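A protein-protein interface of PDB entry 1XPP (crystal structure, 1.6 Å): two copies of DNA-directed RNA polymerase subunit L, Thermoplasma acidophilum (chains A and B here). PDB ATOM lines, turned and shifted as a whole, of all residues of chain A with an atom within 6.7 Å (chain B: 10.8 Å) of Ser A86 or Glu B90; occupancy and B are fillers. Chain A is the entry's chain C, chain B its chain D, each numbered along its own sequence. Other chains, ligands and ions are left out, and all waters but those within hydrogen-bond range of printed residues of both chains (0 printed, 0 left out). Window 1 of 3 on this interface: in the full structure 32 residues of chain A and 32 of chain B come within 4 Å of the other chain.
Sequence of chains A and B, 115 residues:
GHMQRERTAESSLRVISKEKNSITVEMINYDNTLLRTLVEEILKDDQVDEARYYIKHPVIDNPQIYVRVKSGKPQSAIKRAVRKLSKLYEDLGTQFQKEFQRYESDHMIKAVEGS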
ATOM      1  N   ALA A  81      17.230 -19.299  14.052  1.00  0.00           N
ATOM      2  CA  ALA A  81      16.539 -19.844  12.887  1.00  0.00           C
ATOM      3  C   ALA A  81      17.071 -19.231  11.614  1.00  0.00           C
ATOM      4  O   ALA A  81      17.265 -19.930  10.624  1.00  0.00           O
ATOM      5  CB  ALA A  81      15.020 -19.622  12.984  1.00  0.00           C
ATOM      6  N   VAL A  82      17.291 -17.922  11.642  1.00  0.00           N
ATOM      7  CA  VAL A  82      17.680 -17.205  10.417  1.00  0.00           C
ATOM      8  C   VAL A  82      19.111 -17.617  10.071  1.00  0.00           C
ATOM      9  O   VAL A  82      19.463 -17.787   8.882  1.00  0.00           O
ATOM     10  CB  VAL A  82      17.503 -15.662  10.531  1.00  0.00           C
ATOM     11  CG1 VAL A  82      18.129 -14.917   9.345  1.00  0.00           C
ATOM     12  CG2 VAL A  82      15.976 -15.314  10.664  1.00  0.00           C
ATOM     13  N   ARG A  83      19.925 -17.782  11.101  1.00  0.00           N
ATOM     14  CA  ARG A  83      21.311 -18.167  10.912  1.00  0.00           C
ATOM     15  C   ARG A  83      21.389 -19.559  10.324  1.00  0.00           C
ATOM     16  O   ARG A  83      22.172 -19.782   9.408  1.00  0.00           O
ATOM     17  CB  ARG A  83      22.096 -18.123  12.227  1.00  0.00           C
ATOM     18  CG  ARG A  83      22.370 -16.727  12.724  1.00  0.00           C
ATOM     19  CD  ARG A  83      23.274 -16.693  13.963  1.00  0.00           C
ATOM     20  NE  ARG A  83      22.793 -17.559  15.045  1.00  0.00           N
ATOM     21  CZ  ARG A  83      23.443 -18.626  15.502  1.00  0.00           C
ATOM     22  NH1 ARG A  83      24.628 -18.962  14.993  1.00  0.00           N
ATOM     23  NH2 ARG A  83      22.917 -19.352  16.480  1.00  0.00           N
ATOM     24  N   LYS A  84      20.565 -20.480  10.826  1.00  0.00           N
ATOM     25  CA  LYS A  84      20.487 -21.819  10.291  1.00  0.00           C
ATOM     26  C   LYS A  84      20.097 -21.780   8.819  1.00  0.00           C
ATOM     27  O   LYS A  84      20.667 -22.512   8.018  1.00  0.00           O
ATOM     28  CB  LYS A  84      19.481 -22.671  11.043  1.00  0.00           C
ATOM     29  CG  LYS A  84      19.911 -23.200  12.379  1.00  0.00           C
ATOM     30  CD  LYS A  84      18.819 -24.134  12.874  1.00  0.00           C
ATOM     31  CE  LYS A  84      18.369 -23.823  14.284  1.00  0.00           C
ATOM     32  NZ  LYS A  84      17.363 -24.826  14.720  1.00  0.00           N
ATOM     33  N   LEU A  85      19.118 -20.941   8.468  1.00  0.00           N
ATOM     34  CA  LEU A  85      18.616 -20.904   7.084  1.00  0.00           C
ATOM     35  C   LEU A  85      19.650 -20.328   6.113  1.00  0.00           C
ATOM     36  O   LEU A  85      19.860 -20.884   5.013  1.00  0.00           O
ATOM     37  CB  LEU A  85      17.301 -20.126   6.991  1.00  0.00           C
ATOM     38  CG  LEU A  85      16.102 -20.874   7.603  1.00  0.00           C
ATOM     39  CD1 LEU A  85      14.935 -19.905   7.873  1.00  0.00           C
ATOM     40  CD2 LEU A  85      15.664 -21.946   6.648  1.00  0.00           C
ATOM     41  N   SER A  86      20.301 -19.239   6.537  1.00  0.00           N
ATOM     42  CA  SER A  86      21.384 -18.613   5.773  1.00  0.00           C
ATOM     43  C   SER A  86      22.470 -19.649   5.539  1.00  0.00           C
ATOM     44  O   SER A  86      22.931 -19.797   4.411  1.00  0.00           O
ATOM     45  CB  SER A  86      21.962 -17.441   6.595  1.00  0.00           C
ATOM     46  OG  SER A  86      21.011 -16.402   6.607  1.00  0.00           O
ATOM     47  N   LYS A  87      22.842 -20.385   6.590  1.00  0.00           N
ATOM     48  CA  LYS A  87      23.969 -21.335   6.506  1.00  0.00           C
ATOM     49  C   LYS A  87      23.621 -22.495   5.594  1.00  0.00           C
ATOM     50  O   LYS A  87      24.448 -22.928   4.786  1.00  0.00           O
ATOM     51  CB  LYS A  87      24.357 -21.797   7.916  1.00  0.00           C
ATOM     52  CG  LYS A  87      25.498 -22.815   8.054  1.00  0.00           C
ATOM     53  CD  LYS A  87      26.801 -22.336   7.422  1.00  0.00           C
ATOM     54  CE  LYS A  87      28.015 -23.164   7.884  1.00  0.00           C
ATOM     55  NZ  LYS A  87      27.705 -24.623   8.168  1.00  0.00           N
ATOM     56  N   LEU A  88      22.375 -22.956   5.664  1.00  0.00           N
ATOM     57  CA  LEU A  88      21.900 -24.069   4.809  1.00  0.00           C
ATOM     58  C   LEU A  88      22.067 -23.722   3.316  1.00  0.00           C
ATOM     59  O   LEU A  88      22.551 -24.534   2.537  1.00  0.00           O
ATOM     60  CB  LEU A  88      20.416 -24.322   5.109  1.00  0.00           C
ATOM     61  CG  LEU A  88      19.793 -25.716   5.097  1.00  0.00           C
ATOM     62  CD1 LEU A  88      18.337 -25.551   4.732  1.00  0.00           C
ATOM     63  CD2 LEU A  88      20.465 -26.714   4.161  1.00  0.00           C
ATOM     64  N   TYR A  89      21.621 -22.529   2.918  1.00  0.00           N
ATOM     65  CA  TYR A  89      21.764 -22.117   1.510  1.00  0.00           C
ATOM     66  C   TYR A  89      23.197 -21.739   1.125  1.00  0.00           C
ATOM     67  O   TYR A  89      23.608 -21.912  -0.022  1.00  0.00           O
ATOM     68  CB  TYR A  89      20.770 -21.032   1.152  1.00  0.00           C
ATOM     69  CG  TYR A  89      19.409 -21.614   1.012  1.00  0.00           C
ATOM     70  CD1 TYR A  89      19.055 -22.296  -0.144  1.00  0.00           C
ATOM     71  CD2 TYR A  89      18.515 -21.552   2.072  1.00  0.00           C
ATOM     72  CE1 TYR A  89      17.811 -22.893  -0.246  1.00  0.00           C
ATOM     73  CE2 TYR A  89      17.257 -22.135   1.975  1.00  0.00           C
ATOM     74  CZ  TYR A  89      16.919 -22.792   0.817  1.00  0.00           C
ATOM     75  OH  TYR A  89      15.679 -23.367   0.718  1.00  0.00           O
ATOM     76  N   GLU A  90      23.968 -21.188   2.064  1.00  0.00           N
ATOM     77  CA  GLU A  90      25.403 -20.963   1.812  1.00  0.00           C
ATOM     78  C   GLU A  90      26.119 -22.303   1.596  1.00  0.00           C
ATOM     79  O   GLU A  90      26.919 -22.446   0.660  1.00  0.00           O
ATOM     80  CB  GLU A  90      26.045 -20.147   2.961  1.00  0.00           C
ATOM     81  CG  GLU A  90      25.488 -18.719   3.062  1.00  0.00           C
ATOM     82  CD  GLU A  90      25.641 -18.090   4.438  1.00  0.00           C
ATOM     83  OE1 GLU A  90      26.151 -18.739   5.382  1.00  0.00           O
ATOM     84  OE2 GLU A  90      25.183 -16.933   4.563  1.00  0.00           O
ATOM     85  N   ASP A  91      25.812 -23.283   2.437  1.00  0.00           N
ATOM     86  CA  ASP A  91      26.441 -24.587   2.321  1.00  0.00           C
ATOM     87  C   ASP A  91      26.007 -25.284   1.043  1.00  0.00           C
ATOM     88  O   ASP A  91      26.834 -25.912   0.363  1.00  0.00           O
ATOM     89  CB  ASP A  91      26.143 -25.447   3.543  1.00  0.00           C
ATOM     90  CG  ASP A  91      26.870 -24.987   4.785  1.00  0.00           C
ATOM     91  OD1 ASP A  91      27.805 -24.124   4.710  1.00  0.00           O
ATOM     92  OD2 ASP A  91      26.468 -25.499   5.851  1.00  0.00           O
ATOM     93  N   LEU B  34      13.550 -27.481   1.572  1.00  0.00           N
ATOM     94  CA  LEU B  34      14.668 -26.930   0.774  1.00  0.00           C
ATOM     95  C   LEU B  34      14.509 -27.233  -0.729  1.00  0.00           C
ATOM     96  O   LEU B  34      14.659 -26.353  -1.576  1.00  0.00           O
ATOM     97  CB  LEU B  34      16.038 -27.432   1.291  1.00  0.00           C
ATOM     98  CG  LEU B  34      17.217 -26.849   0.468  1.00  0.00           C
ATOM     99  CD1 LEU B  34      18.433 -26.522   1.320  1.00  0.00           C
ATOM    100  CD2 LEU B  34      17.591 -27.814  -0.600  1.00  0.00           C
ATOM    101  N   ALA B  81      19.769 -19.373  -8.578  1.00  0.00           N
ATOM    102  CA  ALA B  81      18.732 -19.539  -7.569  1.00  0.00           C
ATOM    103  C   ALA B  81      19.275 -19.730  -6.174  1.00  0.00           C
ATOM    104  O   ALA B  81      18.722 -19.154  -5.217  1.00  0.00           O
ATOM    105  CB  ALA B  81      17.819 -20.705  -7.918  1.00  0.00           C
ATOM    106  N   VAL B  82      20.305 -20.578  -6.029  1.00  0.00           N
ATOM    107  CA  VAL B  82      20.929 -20.820  -4.714  1.00  0.00           C
ATOM    108  C   VAL B  82      21.488 -19.498  -4.182  1.00  0.00           C
ATOM    109  O   VAL B  82      21.276 -19.156  -3.018  1.00  0.00           O
ATOM    110  CB  VAL B  82      22.050 -21.871  -4.781  1.00  0.00           C
ATOM    111  CG1 VAL B  82      22.748 -21.988  -3.466  1.00  0.00           C
ATOM    112  CG2 VAL B  82      21.437 -23.225  -5.183  1.00  0.00           C
ATOM    113  N   ARG B  83      22.176 -18.763  -5.035  1.00  0.00           N
ATOM    114  CA  ARG B  83      22.774 -17.491  -4.563  1.00  0.00           C
ATOM    115  C   ARG B  83      21.669 -16.489  -4.195  1.00  0.00           C
ATOM    116  O   ARG B  83      21.832 -15.716  -3.217  1.00  0.00           O
ATOM    117  CB  ARG B  83      23.758 -16.904  -5.586  1.00  0.00           C
ATOM    118  CG  ARG B  83      24.927 -17.854  -5.967  1.00  0.00           C
ATOM    119  CD  ARG B  83      25.974 -18.109  -4.846  1.00  0.00           C
ATOM    120  NE  ARG B  83      26.711 -19.372  -5.040  1.00  0.00           N
ATOM    121  CZ  ARG B  83      27.914 -19.626  -4.529  1.00  0.00           C
ATOM    122  NH1 ARG B  83      28.544 -18.681  -3.827  1.00  0.00           N
ATOM    123  NH2 ARG B  83      28.495 -20.809  -4.727  1.00  0.00           N
ATOM    124  N   LYS B  84      20.568 -16.444  -4.950  1.00  0.00           N
ATOM    125  CA  LYS B  84      19.459 -15.539  -4.567  1.00  0.00           C
ATOM    126  C   LYS B  84      18.912 -15.929  -3.202  1.00  0.00           C
ATOM    127  O   LYS B  84      18.653 -15.067  -2.351  1.00  0.00           O
ATOM    128  CB  LYS B  84      18.328 -15.577  -5.597  1.00  0.00           C
ATOM    129  CG  LYS B  84      18.635 -14.875  -6.900  1.00  0.00           C
ATOM    130  CD  LYS B  84      17.348 -14.737  -7.700  1.00  0.00           C
ATOM    131  CE  LYS B  84      17.553 -14.982  -9.181  1.00  0.00           C
ATOM    132  NZ  LYS B  84      16.236 -15.204  -9.890  1.00  0.00           N
ATOM    133  N   LEU B  85      18.736 -17.231  -2.979  1.00  0.00           N
ATOM    134  CA  LEU B  85      18.169 -17.715  -1.719  1.00  0.00           C
ATOM    135  C   LEU B  85      19.074 -17.424  -0.514  1.00  0.00           C
ATOM    136  O   LEU B  85      18.596 -17.027   0.549  1.00  0.00           O
ATOM    137  CB  LEU B  85      17.855 -19.211  -1.788  1.00  0.00           C
ATOM    138  CG  LEU B  85      16.631 -19.482  -2.680  1.00  0.00           C
ATOM    139  CD1 LEU B  85      16.522 -20.987  -2.944  1.00  0.00           C
ATOM    140  CD2 LEU B  85      15.327 -18.969  -2.117  1.00  0.00           C
ATOM    141  N   SER B  86      20.377 -17.595  -0.708  1.00  0.00           N
ATOM    142  CA  SER B  86      21.346 -17.277   0.331  1.00  0.00           C
ATOM    143  C   SER B  86      21.217 -15.804   0.681  1.00  0.00           C
ATOM    144  O   SER B  86      21.182 -15.431   1.877  1.00  0.00           O
ATOM    145  CB  SER B  86      22.736 -17.558  -0.250  1.00  0.00           C
ATOM    146  OG  SER B  86      22.870 -18.972  -0.449  1.00  0.00           O
ATOM    147  N   LYS B  87      21.121 -14.960  -0.343  1.00  0.00           N
ATOM    148  CA  LYS B  87      20.994 -13.506  -0.098  1.00  0.00           C
ATOM    149  C   LYS B  87      19.699 -13.155   0.613  1.00  0.00           C
ATOM    150  O   LYS B  87      19.688 -12.306   1.514  1.00  0.00           O
ATOM    151  CB  LYS B  87      21.075 -12.738  -1.403  1.00  0.00           C
ATOM    152  CG  LYS B  87      20.877 -11.239  -1.219  1.00  0.00           C
ATOM    153  CD  LYS B  87      21.033 -10.470  -2.504  1.00  0.00           C
ATOM    154  CE  LYS B  87      20.711  -9.004  -2.266  1.00  0.00           C
ATOM    155  NZ  LYS B  87      21.411  -8.487  -1.071  1.00  0.00           N
ATOM    156  N   LEU B  88      18.604 -13.801   0.216  1.00  0.00           N
ATOM    157  CA  LEU B  88      17.296 -13.546   0.858  1.00  0.00           C
ATOM    158  C   LEU B  88      17.351 -13.756   2.378  1.00  0.00           C
ATOM    159  O   LEU B  88      16.915 -12.885   3.143  1.00  0.00           O
ATOM    160  CB  LEU B  88      16.188 -14.440   0.236  1.00  0.00           C
ATOM    161  CG  LEU B  88      15.546 -13.885  -1.053  1.00  0.00           C
ATOM    162  CD1 LEU B  88      14.805 -15.011  -1.749  1.00  0.00           C
ATOM    163  CD2 LEU B  88      14.552 -12.762  -0.758  1.00  0.00           C
ATOM    164  N   TYR B  89      17.860 -14.902   2.806  1.00  0.00           N
ATOM    165  CA  TYR B  89      17.952 -15.249   4.233  1.00  0.00           C
ATOM    166  C   TYR B  89      19.026 -14.416   4.942  1.00  0.00           C
ATOM    167  O   TYR B  89      18.819 -13.958   6.089  1.00  0.00           O
ATOM    168  CB  TYR B  89      18.159 -16.752   4.444  1.00  0.00           C
ATOM    169  CG  TYR B  89      16.902 -17.550   4.086  1.00  0.00           C
ATOM    170  CD1 TYR B  89      16.868 -18.324   2.930  1.00  0.00           C
ATOM    171  CD2 TYR B  89      15.787 -17.545   4.936  1.00  0.00           C
ATOM    172  CE1 TYR B  89      15.741 -19.057   2.598  1.00  0.00           C
ATOM    173  CE2 TYR B  89      14.628 -18.257   4.596  1.00  0.00           C
ATOM    174  CZ  TYR B  89      14.616 -19.004   3.449  1.00  0.00           C
ATOM    175  OH  TYR B  89      13.500 -19.754   3.116  1.00  0.00           O
ATOM    176  N   GLU B  90      20.126 -14.150   4.251  1.00  0.00           N
ATOM    177  CA  GLU B  90      21.146 -13.270   4.837  1.00  0.00           C
ATOM    178  C   GLU B  90      20.587 -11.888   5.110  1.00  0.00           C
ATOM    179  O   GLU B  90      20.792 -11.342   6.202  1.00  0.00           O
ATOM    180  CB  GLU B  90      22.381 -13.210   3.931  1.00  0.00           C
ATOM    181  CG  GLU B  90      23.237 -14.475   3.955  1.00  0.00           C
ATOM    182  CD  GLU B  90      24.164 -14.533   2.726  1.00  0.00           C
ATOM    183  OE1 GLU B  90      24.122 -13.624   1.865  1.00  0.00           O
ATOM    184  OE2 GLU B  90      24.917 -15.515   2.600  1.00  0.00           O
ATOM    185  N   ASP B  91      19.885 -11.339   4.117  1.00  0.00           N
ATOM    186  CA  ASP B  91      19.314  -9.980   4.201  1.00  0.00           C
ATOM    187  C   ASP B  91      18.244  -9.968   5.285  1.00  0.00           C
ATOM    188  O   ASP B  91      18.124  -9.006   6.061  1.00  0.00           O
ATOM    189  CB  ASP B  91      18.727  -9.520   2.878  1.00  0.00           C
ATOM    190  CG  ASP B  91      19.797  -9.161   1.821  1.00  0.00           C
ATOM    191  OD1 ASP B  91      21.008  -9.103   2.159  1.00  0.00           O
ATOM    192  OD2 ASP B  91      19.385  -8.860   0.687  1.00  0.00           O
ATOM    193  N   LEU B  92      17.486 -11.057   5.352  1.00  0.00           N
ATOM    194  CA  LEU B  92      16.478 -11.188   6.412  1.00  0.00           C
ATOM    195  C   LEU B  92      17.151 -11.033   7.791  1.00  0.00           C
ATOM    196  O   LEU B  92      16.668 -10.269   8.644  1.00  0.00           O
ATOM    197  CB  LEU B  92      15.755 -12.530   6.298  1.00  0.00           C
ATOM    198  CG  LEU B  92      14.719 -12.842   7.382  1.00  0.00           C
ATOM    199  CD1 LEU B  92      13.529 -11.851   7.315  1.00  0.00           C
ATOM    200  CD2 LEU B  92      14.285 -14.295   7.309  1.00  0.00           C
ATOM    201  N   GLY B  93      18.257 -11.740   8.015  1.00  0.00           N
ATOM    202  CA  GLY B  93      18.979 -11.618   9.290  1.00  0.00           C
ATOM    203  C   GLY B  93      19.560 -10.227   9.526  1.00  0.00           C
ATOM    204  O   GLY B  93      19.520  -9.737  10.652  1.00  0.00           O
ATOM    205  N   THR B  94      20.067  -9.574   8.487  1.00  0.00           N
ATOM    206  CA  THR B  94      20.577  -8.206   8.626  1.00  0.00           C
ATOM    207  C   THR B  94      19.469  -7.283   9.091  1.00  0.00           C
ATOM    208  O   THR B  94      19.661  -6.457  10.003  1.00  0.00           O
ATOM    209  CB  THR B  94      21.141  -7.706   7.321  1.00  0.00           C
ATOM    210  OG1 THR B  94      22.227  -8.588   6.998  1.00  0.00           O
ATOM    211  CG2 THR B  94      21.666  -6.267   7.475  1.00  0.00           C
ATOM    212  N   GLN B  95      18.293  -7.465   8.514  1.00  0.00           N
ATOM    213  CA  GLN B  95      17.143  -6.616   8.884  1.00  0.00           C
ATOM    214  C   GLN B  95      16.681  -6.865  10.318  1.00  0.00           C
ATOM    215  O   GLN B  95      16.469  -5.903  11.071  1.00  0.00           O
ATOM    216  CB  GLN B  95      15.995  -6.817   7.892  1.00  0.00           C
ATOM    217  CG  GLN B  95      16.326  -6.242   6.559  1.00  0.00           C
ATOM    218  CD  GLN B  95      15.133  -5.805   5.781  1.00  0.00           C
ATOM    219  OE1 GLN B  95      14.027  -6.348   5.960  1.00  0.00           O
ATOM    220  NE2 GLN B  95      15.317  -4.804   4.926  1.00  0.00           N
ATOM    221  N   PHE B  96      16.517  -8.128  10.705  1.00  0.00           N
ATOM    222  CA  PHE B  96      16.195  -8.480  12.087  1.00  0.00           C
ATOM    223  C   PHE B  96      17.238  -7.894  13.058  1.00  0.00           C
ATOM    224  O   PHE B  96      16.875  -7.297  14.065  1.00  0.00           O
ATOM    225  CB  PHE B  96      16.118  -9.991  12.276  1.00  0.00           C
ATOM    226  CG  PHE B  96      14.753 -10.601  12.007  1.00  0.00           C
ATOM    227  CD1 PHE B  96      13.613 -10.184  12.712  1.00  0.00           C
ATOM    228  CD2 PHE B  96      14.633 -11.646  11.092  1.00  0.00           C
ATOM    229  CE1 PHE B  96      12.355 -10.784  12.484  1.00  0.00           C
ATOM    230  CE2 PHE B  96      13.390 -12.265  10.862  1.00  0.00           C
ATOM    231  CZ  PHE B  96      12.224 -11.822  11.553  1.00  0.00           C
ATOM    232  N   GLN B  97      18.515  -8.263  12.877  1.00  0.00           N
ATOM    233  CA  GLN B  97      19.502  -8.036  13.942  1.00  0.00           C
ATOM    234  C   GLN B  97      19.592  -6.548  14.187  1.00  0.00           C
ATOM    235  O   GLN B  97      19.784  -6.097  15.326  1.00  0.00           O
ATOM    236  CB  GLN B  97      20.887  -8.618  13.604  1.00  0.00           C
ATOM    237  CG  GLN B  97      21.017 -10.121  13.830  1.00  0.00           C
ATOM    238  CD  GLN B  97      20.900 -10.550  15.302  1.00  0.00           C
ATOM    239  OE1 GLN B  97      21.729 -10.197  16.143  1.00  0.00           O
ATOM    240  NE2 GLN B  97      19.885 -11.352  15.600  1.00  0.00           N
ATOM    241  N   LYS B  98      19.408  -5.779  13.120  1.00  0.00           N
ATOM    242  CA  LYS B  98      19.502  -4.331  13.238  1.00  0.00           C
ATOM    243  C   LYS B  98      18.354  -3.850  14.055  1.00  0.00           C
ATOM    244  O   LYS B  98      18.480  -2.914  14.851  1.00  0.00           O
ATOM    245  CB  LYS B  98      19.456  -3.652  11.884  1.00  0.00           C
ATOM    246  CG  LYS B  98      19.832  -2.173  11.943  1.00  0.00           C
ATOM    247  CD  LYS B  98      19.317  -1.405  10.731  1.00  0.00           C
ATOM    248  CE  LYS B  98      20.012  -1.799   9.425  1.00  0.00           C
ATOM    249  NZ  LYS B  98      19.318  -1.125   8.280  1.00  0.00           N
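OG of Ser A86 sits close to O of Tyr B89 (3.3 Å). OG of Ser A86 is in hydrogen-bond range of N of Glu B90, 3.4 Å away. OE2 of Glu B90 lies close to OE2 of Glu A90, at 2.4 Å. The backbone carbonyl oxygen (O) of Tyr A89 is in hydrogen-bond range of the side-chain hydroxyl (OG) of Ser B86.
O of Val B82 sits at hydrogen-bond distance from OG of Ser B86 (3.0 Å). O of Glu B90 sits at hydrogen-bond distance from OG1 of Thr B94, at 3.2 Å. The backbone carbonyl oxygen (O) of Val A82 is in hydrogen-bond range of the side-chain hydroxyl (OG) of Ser A86 (3.1 Å).
Among the printed residues, merely in contact across the chains: Val A82 with Tyr B89, Val A82 with Leu B92, Val A82 with Gly B93, Val A82 with Phe B96, Leu A85 with Tyr B89, Leu A88 with Leu B34, Tyr A89 with Leu B34, Tyr A89 with Val B82, Tyr A89 with Leu B85, Tyr A89 with Tyr B89 and Glu A90 with Ser B86.
Printed residues of chain B within 4 Å of Leu A85: Tyr B89 (3.6 Å). Ser A86 touches just these residues of chain B: Tyr B89 and Glu B90. Printed residues of chain B within 4 Å of Leu A88: Leu B34. Of the printed residues of chain B, Tyr A89 touches Leu B34, Val B82, Leu B85, Ser B86 and Tyr B89. Of chain B, only Ser B86 (3.5 Å) and Glu B90 (2.4 Å) come within 4 Å of Glu A90. Printed residues of chain A within 4 Å of Leu B34: Leu A88 and Tyr A89. Of the printed residues of chain A, Leu B85 touches Tyr A89 (3.5 Å). Printed residues of chain A within 4 Å of Ser B86: Tyr A89 (3.1 Å) and Glu A90 (3.5 Å). Printed residues of chain A within 4 Å of Glu B90: Ser A86 and Glu A90. The nearest residue of chain A that does not touch Glu B90 is Val A82 (5.5 Å). The nearest printed residue of chain A that does not touch Leu B85 is Leu A85 (6.0 Å).
Of the 11 printed residues of chain A, 6 touch a printed residue of chain B. Printed residues of chain A that touch a printed residue of chain B: Val A82, Leu A85, Ser A86, Leu A88, Tyr A89 and Glu A90. Hydrophobic or aromatic side chains of chain B that line the printed part of chain A: Leu B34, Val B82, Leu B85, Tyr B89, Leu B92 and Phe B96. Among the printed residues, 15 pairs touch across the chains.
Val A82 touches Tyr B89, and with the chains exchanged Tyr A89 touches Val B82. Leu A85 touches Tyr B89, and with the chains exchanged Tyr A89 touches Leu B85. Ser A86 touches Tyr B89, and with the chains exchanged Tyr A89 touches Ser B86. Glu B90 touches its own counterpart, Glu A90.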
